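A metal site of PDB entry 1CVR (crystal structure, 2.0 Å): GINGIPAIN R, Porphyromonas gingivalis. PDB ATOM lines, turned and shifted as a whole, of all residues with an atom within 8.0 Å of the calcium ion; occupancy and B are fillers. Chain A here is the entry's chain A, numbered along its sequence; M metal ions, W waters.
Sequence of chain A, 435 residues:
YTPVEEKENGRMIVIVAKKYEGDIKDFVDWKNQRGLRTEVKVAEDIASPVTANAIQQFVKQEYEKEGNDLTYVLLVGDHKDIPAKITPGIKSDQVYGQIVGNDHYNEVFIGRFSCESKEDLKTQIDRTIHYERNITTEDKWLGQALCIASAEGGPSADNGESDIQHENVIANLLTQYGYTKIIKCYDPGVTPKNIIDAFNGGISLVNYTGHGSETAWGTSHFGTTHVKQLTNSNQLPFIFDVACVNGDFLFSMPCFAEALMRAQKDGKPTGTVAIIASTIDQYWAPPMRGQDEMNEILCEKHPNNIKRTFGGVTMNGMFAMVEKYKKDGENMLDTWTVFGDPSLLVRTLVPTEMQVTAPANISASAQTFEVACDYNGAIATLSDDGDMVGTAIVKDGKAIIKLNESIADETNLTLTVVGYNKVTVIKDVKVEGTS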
ATOM      1  N   GLY A  77     -16.355  18.901  10.833  1.00  0.00           N
ATOM      2  CA  GLY A  77     -15.878  17.602  10.386  1.00  0.00           C
ATOM      3  C   GLY A  77     -14.766  17.809   9.370  1.00  0.00           C
ATOM      4  O   GLY A  77     -14.618  18.935   8.867  1.00  0.00           O
ATOM      5  N   ASP A  78     -13.974  16.770   9.066  1.00  0.00           N
ATOM      6  CA  ASP A  78     -12.918  16.898   8.035  1.00  0.00           C
ATOM      7  C   ASP A  78     -13.630  16.547   6.703  1.00  0.00           C
ATOM      8  O   ASP A  78     -14.848  16.350   6.715  1.00  0.00           O
ATOM      9  CB  ASP A  78     -11.746  15.950   8.366  1.00  0.00           C
ATOM     10  CG  ASP A  78     -10.424  16.329   7.660  1.00  0.00           C
ATOM     11  OD1 ASP A  78      -9.336  16.110   8.243  1.00  0.00           O
ATOM     12  OD2 ASP A  78     -10.462  16.826   6.516  1.00  0.00           O
ATOM     13  N   HIS A  79     -12.908  16.505   5.578  1.00  0.00           N
ATOM     14  CA  HIS A  79     -13.514  16.232   4.262  1.00  0.00           C
ATOM     15  C   HIS A  79     -14.305  14.941   4.172  1.00  0.00           C
ATOM     16  O   HIS A  79     -15.295  14.879   3.445  1.00  0.00           O
ATOM     17  CB  HIS A  79     -12.450  16.199   3.140  1.00  0.00           C
ATOM     18  CG  HIS A  79     -12.982  15.756   1.797  1.00  0.00           C
ATOM     19  ND1 HIS A  79     -13.771  16.554   0.996  1.00  0.00           N
ATOM     20  CD2 HIS A  79     -12.887  14.553   1.159  1.00  0.00           C
ATOM     21  CE1 HIS A  79     -14.150  15.870  -0.079  1.00  0.00           C
ATOM     22  NE2 HIS A  79     -13.620  14.652   0.000  1.00  0.00           N
ATOM     23  N   LYS A  80     -13.869  13.919   4.887  1.00  0.00           N
ATOM     24  CA  LYS A  80     -14.568  12.651   4.866  1.00  0.00           C
ATOM     25  C   LYS A  80     -15.924  12.736   5.581  1.00  0.00           C
ATOM     26  O   LYS A  80     -16.846  12.011   5.252  1.00  0.00           O
ATOM     27  CB  LYS A  80     -13.680  11.580   5.525  1.00  0.00           C
ATOM     28  CG  LYS A  80     -14.197  10.144   5.433  1.00  0.00           C
ATOM     29  CD  LYS A  80     -13.147   9.165   5.986  1.00  0.00           C
ATOM     30  CE  LYS A  80     -13.611   7.711   5.919  1.00  0.00           C
ATOM     31  NZ  LYS A  80     -12.578   6.758   6.453  1.00  0.00           N
ATOM     32  N   ARG A 112     -14.970  26.336   8.773  1.00  0.00           N
ATOM     33  CA  ARG A 112     -14.942  24.908   9.125  1.00  0.00           C
ATOM     34  C   ARG A 112     -14.056  24.562  10.313  1.00  0.00           C
ATOM     35  O   ARG A 112     -12.950  25.088  10.459  1.00  0.00           O
ATOM     36  CB  ARG A 112     -14.478  24.072   7.913  1.00  0.00           C
ATOM     37  CG  ARG A 112     -14.218  22.566   8.169  1.00  0.00           C
ATOM     38  CD  ARG A 112     -13.626  21.872   6.929  1.00  0.00           C
ATOM     39  NE  ARG A 112     -14.499  21.822   5.747  1.00  0.00           N
ATOM     40  CZ  ARG A 112     -15.240  20.768   5.369  1.00  0.00           C
ATOM     41  NH1 ARG A 112     -15.228  19.644   6.081  1.00  0.00           N
ATOM     42  NH2 ARG A 112     -15.940  20.817   4.236  1.00  0.00           N
ATOM     43  N   SER A 114     -12.228  21.627  11.165  1.00  0.00           N
ATOM     44  CA  SER A 114     -11.798  20.332  10.629  1.00  0.00           C
ATOM     45  C   SER A 114     -11.314  19.458  11.780  1.00  0.00           C
ATOM     46  O   SER A 114     -10.337  19.802  12.469  1.00  0.00           O
ATOM     47  CB  SER A 114     -10.678  20.519   9.613  1.00  0.00           C
ATOM     48  OG  SER A 114     -10.182  19.247   9.216  1.00  0.00           O
ATOM     49  N   CYS A 115     -11.983  18.326  11.977  1.00  0.00           N
ATOM     50  CA  CYS A 115     -11.675  17.404  13.078  1.00  0.00           C
ATOM     51  C   CYS A 115     -11.663  15.950  12.632  1.00  0.00           C
ATOM     52  O   CYS A 115     -12.484  15.542  11.802  1.00  0.00           O
ATOM     53  CB  CYS A 115     -12.745  17.481  14.154  1.00  0.00           C
ATOM     54  SG  CYS A 115     -13.305  19.097  14.582  1.00  0.00           S
ATOM     55  N   GLU A 116     -10.766  15.153  13.204  1.00  0.00           N
ATOM     56  CA  GLU A 116     -10.739  13.733  12.899  1.00  0.00           C
ATOM     57  C   GLU A 116     -10.907  12.969  14.223  1.00  0.00           C
ATOM     58  O   GLU A 116     -10.932  11.738  14.244  1.00  0.00           O
ATOM     59  CB  GLU A 116      -9.432  13.357  12.183  1.00  0.00           C
ATOM     60  CG  GLU A 116      -9.280  14.048  10.825  1.00  0.00           C
ATOM     61  CD  GLU A 116      -8.011  13.671  10.077  1.00  0.00           C
ATOM     62  OE1 GLU A 116      -8.006  12.629   9.384  1.00  0.00           O
ATOM     63  OE2 GLU A 116      -7.010  14.410  10.170  1.00  0.00           O
ATOM     64  N   GLY A 247      -3.831  25.291   2.816  1.00  0.00           N
ATOM     65  CA  GLY A 247      -5.145  24.885   3.285  1.00  0.00           C
ATOM     66  C   GLY A 247      -5.760  23.674   2.610  1.00  0.00           C
ATOM     67  O   GLY A 247      -6.971  23.482   2.681  1.00  0.00           O
ATOM     68  N   ASP A 248      -4.942  22.831   1.973  1.00  0.00           N
ATOM     69  CA  ASP A 248      -5.493  21.649   1.306  1.00  0.00           C
ATOM     70  C   ASP A 248      -5.864  20.602   2.347  1.00  0.00           C
ATOM     71  O   ASP A 248      -5.056  19.704   2.688  1.00  0.00           O
ATOM     72  CB  ASP A 248      -4.501  21.091   0.282  1.00  0.00           C
ATOM     73  CG  ASP A 248      -5.005  19.802  -0.377  1.00  0.00           C
ATOM     74  OD1 ASP A 248      -6.219  19.564  -0.399  1.00  0.00           O
ATOM     75  OD2 ASP A 248      -4.167  19.028  -0.886  1.00  0.00           O
ATOM     76  N   PHE A 249      -7.097  20.704   2.851  1.00  0.00           N
ATOM     77  CA  PHE A 249      -7.523  19.774   3.881  1.00  0.00           C
ATOM     78  C   PHE A 249      -7.954  18.417   3.393  1.00  0.00           C
ATOM     79  O   PHE A 249      -8.441  17.596   4.180  1.00  0.00           O
ATOM     80  CB  PHE A 249      -8.600  20.393   4.799  1.00  0.00           C
ATOM     81  CG  PHE A 249      -9.897  20.737   4.107  1.00  0.00           C
ATOM     82  CD1 PHE A 249     -10.007  21.850   3.286  1.00  0.00           C
ATOM     83  CD2 PHE A 249     -11.030  19.953   4.328  1.00  0.00           C
ATOM     84  CE1 PHE A 249     -11.236  22.188   2.687  1.00  0.00           C
ATOM     85  CE2 PHE A 249     -12.237  20.270   3.728  1.00  0.00           C
ATOM     86  CZ  PHE A 249     -12.347  21.393   2.910  1.00  0.00           C
ATOM     87  N   LEU A 250      -7.788  18.174   2.105  1.00  0.00           N
ATOM     88  CA  LEU A 250      -8.105  16.876   1.516  1.00  0.00           C
ATOM     89  C   LEU A 250      -6.792  16.100   1.338  1.00  0.00           C
ATOM     90  O   LEU A 250      -6.793  15.016   0.760  1.00  0.00           O
ATOM     91  CB  LEU A 250      -8.805  17.029   0.161  1.00  0.00           C
ATOM     92  CG  LEU A 250     -10.278  17.468   0.169  1.00  0.00           C
ATOM     93  CD1 LEU A 250     -10.406  18.903   0.647  1.00  0.00           C
ATOM     94  CD2 LEU A 250     -10.828  17.356  -1.242  1.00  0.00           C
ATOM     95  N   PHE A 251      -5.681  16.656   1.825  1.00  0.00           N
ATOM     96  CA  PHE A 251      -4.361  16.029   1.747  1.00  0.00           C
ATOM     97  C   PHE A 251      -4.329  14.744   2.589  1.00  0.00           C
ATOM     98  O   PHE A 251      -5.109  14.606   3.538  1.00  0.00           O
ATOM     99  CB  PHE A 251      -3.311  17.035   2.257  1.00  0.00           C
ATOM    100  CG  PHE A 251      -1.876  16.613   1.999  1.00  0.00           C
ATOM    101  CD1 PHE A 251      -1.456  16.265   0.716  1.00  0.00           C
ATOM    102  CD2 PHE A 251      -0.960  16.609   3.043  1.00  0.00           C
ATOM    103  CE1 PHE A 251      -0.121  15.911   0.476  1.00  0.00           C
ATOM    104  CE2 PHE A 251       0.377  16.252   2.816  1.00  0.00           C
ATOM    105  CZ  PHE A 251       0.789  15.905   1.527  1.00  0.00           C
ATOM    106  N   SER A 252      -3.435  13.804   2.263  1.00  0.00           N
ATOM    107  CA  SER A 252      -3.331  12.539   2.997  1.00  0.00           C
ATOM    108  C   SER A 252      -2.932  12.678   4.465  1.00  0.00           C
ATOM    109  O   SER A 252      -3.102  11.751   5.255  1.00  0.00           O
ATOM    110  CB  SER A 252      -2.355  11.591   2.289  1.00  0.00           C
ATOM    111  OG  SER A 252      -1.053  12.152   2.235  1.00  0.00           O
ATOM    112  N   MET A 253      -2.388  13.840   4.832  1.00  0.00           N
ATOM    113  CA  MET A 253      -2.009  14.103   6.226  1.00  0.00           C
ATOM    114  C   MET A 253      -2.597  15.468   6.587  1.00  0.00           C
ATOM    115  O   MET A 253      -2.989  16.235   5.706  1.00  0.00           O
ATOM    116  CB  MET A 253      -0.488  14.148   6.377  1.00  0.00           C
ATOM    117  CG  MET A 253       0.229  12.891   5.926  1.00  0.00           C
ATOM    118  SD  MET A 253       2.010  13.021   6.141  1.00  0.00           S
ATOM    119  CE  MET A 253       2.403  14.474   5.136  1.00  0.00           C
ATOM    120  N   PRO A 254      -2.679  15.790   7.887  1.00  0.00           N
ATOM    121  CA  PRO A 254      -3.236  17.114   8.210  1.00  0.00           C
ATOM    122  C   PRO A 254      -2.426  18.210   7.511  1.00  0.00           C
ATOM    123  O   PRO A 254      -1.192  18.164   7.511  1.00  0.00           O
ATOM    124  CB  PRO A 254      -3.104  17.163   9.739  1.00  0.00           C
ATOM    125  CG  PRO A 254      -3.272  15.668  10.111  1.00  0.00           C
ATOM    126  CD  PRO A 254      -2.297  15.071   9.116  1.00  0.00           C
ATOM    127  N   CYS A 255      -3.100  19.159   6.872  1.00  0.00           N
ATOM    128  CA  CYS A 255      -2.385  20.254   6.214  1.00  0.00           C
ATOM    129  C   CYS A 255      -1.950  21.283   7.246  1.00  0.00           C
ATOM    130  O   CYS A 255      -2.321  21.217   8.414  1.00  0.00           O
ATOM    131  CB  CYS A 255      -3.260  20.932   5.140  1.00  0.00           C
ATOM    132  SG  CYS A 255      -4.783  21.782   5.721  1.00  0.00           S
ATOM    133  N   GLU A 258      -4.852  22.887   9.236  1.00  0.00           N
ATOM    134  CA  GLU A 258      -5.480  21.989  10.189  1.00  0.00           C
ATOM    135  C   GLU A 258      -4.612  21.752  11.432  1.00  0.00           C
ATOM    136  O   GLU A 258      -5.134  21.705  12.536  1.00  0.00           O
ATOM    137  CB  GLU A 258      -5.783  20.638   9.531  1.00  0.00           C
ATOM    138  CG  GLU A 258      -6.821  20.700   8.431  1.00  0.00           C
ATOM    139  CD  GLU A 258      -7.014  19.350   7.729  1.00  0.00           C
ATOM    140  OE1 GLU A 258      -6.036  18.826   7.139  1.00  0.00           O
ATOM    141  OE2 GLU A 258      -8.142  18.835   7.766  1.00  0.00           O
ATOM    142  N   ARG A 262      -5.737  22.550  15.388  1.00  0.00           N
ATOM    143  CA  ARG A 262      -5.872  21.402  16.304  1.00  0.00           C
ATOM    144  C   ARG A 262      -4.797  21.300  17.396  1.00  0.00           C
ATOM    145  O   ARG A 262      -4.913  20.473  18.311  1.00  0.00           O
ATOM    146  CB  ARG A 262      -5.830  20.103  15.491  1.00  0.00           C
ATOM    147  CG  ARG A 262      -6.921  19.955  14.435  1.00  0.00           C
ATOM    148  CD  ARG A 262      -6.667  18.711  13.573  1.00  0.00           C
ATOM    149  NE  ARG A 262      -7.719  18.503  12.584  1.00  0.00           N
ATOM    150  CZ  ARG A 262      -7.755  17.485  11.734  1.00  0.00           C
ATOM    151  NH1 ARG A 262      -6.793  16.574  11.748  1.00  0.00           N
ATOM    152  NH2 ARG A 262      -8.753  17.368  10.867  1.00  0.00           N
ATOM    153  N   PHE A 339     -10.654  28.358   8.129  1.00  0.00           N
ATOM    154  CA  PHE A 339     -10.582  27.293   9.117  1.00  0.00           C
ATOM    155  C   PHE A 339     -10.811  28.028  10.425  1.00  0.00           C
ATOM    156  O   PHE A 339     -10.069  28.963  10.784  1.00  0.00           O
ATOM    157  CB  PHE A 339      -9.206  26.598   9.131  1.00  0.00           C
ATOM    158  CG  PHE A 339      -8.887  25.859   7.869  1.00  0.00           C
ATOM    159  CD1 PHE A 339      -8.437  26.528   6.734  1.00  0.00           C
ATOM    160  CD2 PHE A 339      -9.046  24.476   7.805  1.00  0.00           C
ATOM    161  CE1 PHE A 339      -8.144  25.849   5.559  1.00  0.00           C
ATOM    162  CE2 PHE A 339      -8.761  23.769   6.616  1.00  0.00           C
ATOM    163  CZ  PHE A 339      -8.309  24.454   5.500  1.00  0.00           C
HETATM  164 CA    CA M   1      -7.934  16.843   6.568  1.00  0.00          CA
HETATM  165  O   HOH W   1      -8.310  14.594   5.483  1.00  0.00           O
HETATM  166  O   HOH W   2      -6.424  15.625   8.046  1.00  0.00           O
HETATM  167  O   HOH W   3      -5.792  16.748   5.394  1.00  0.00           O
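Of the 20 residues printed, 3 come within 4 Å of the calcium ion.
The nearest printed residue that does not touch the calcium ion is Ser 114 (4.2 Å).
The calcium ion is bound by the side-chain carboxylate (OD1) of Asp 78, the side-chain carboxylate (OE2) of Glu 258, water W2, water W3, water W1, the side-chain carboxylate (OD2) of Asp 78, the backbone carbonyl oxygen (O) of Phe 249 and the side-chain carboxylate (OE1) of Glu 258.
O of Cys 115 lies within hydrogen-bond range of N of Asp 78, 3.3 Å away.
NH2 of Arg 262 sits close to OD1 of Asp 78.
The side-chain carboxylate (OE2) of Glu 258 sits close to the guanidinium group (NH2) of Arg 262, 3.5 Å away.
The side-chain carboxylate (OD1) of Asp 78 sits close to the side-chain hydroxyl (OG) of Ser 114, at 3.4 Å.
The side-chain carboxylate of Glu 258 lies close to the side-chain hydroxyl of Ser 114 (2.5 Å).
The backbone NH (N) of Glu 258 sits close to the side-chain sulfur (SG) of Cys 255.
The backbone carbonyl oxygen of Asp 78 is in hydrogen-bond range of the guanidinium group of Arg 112.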
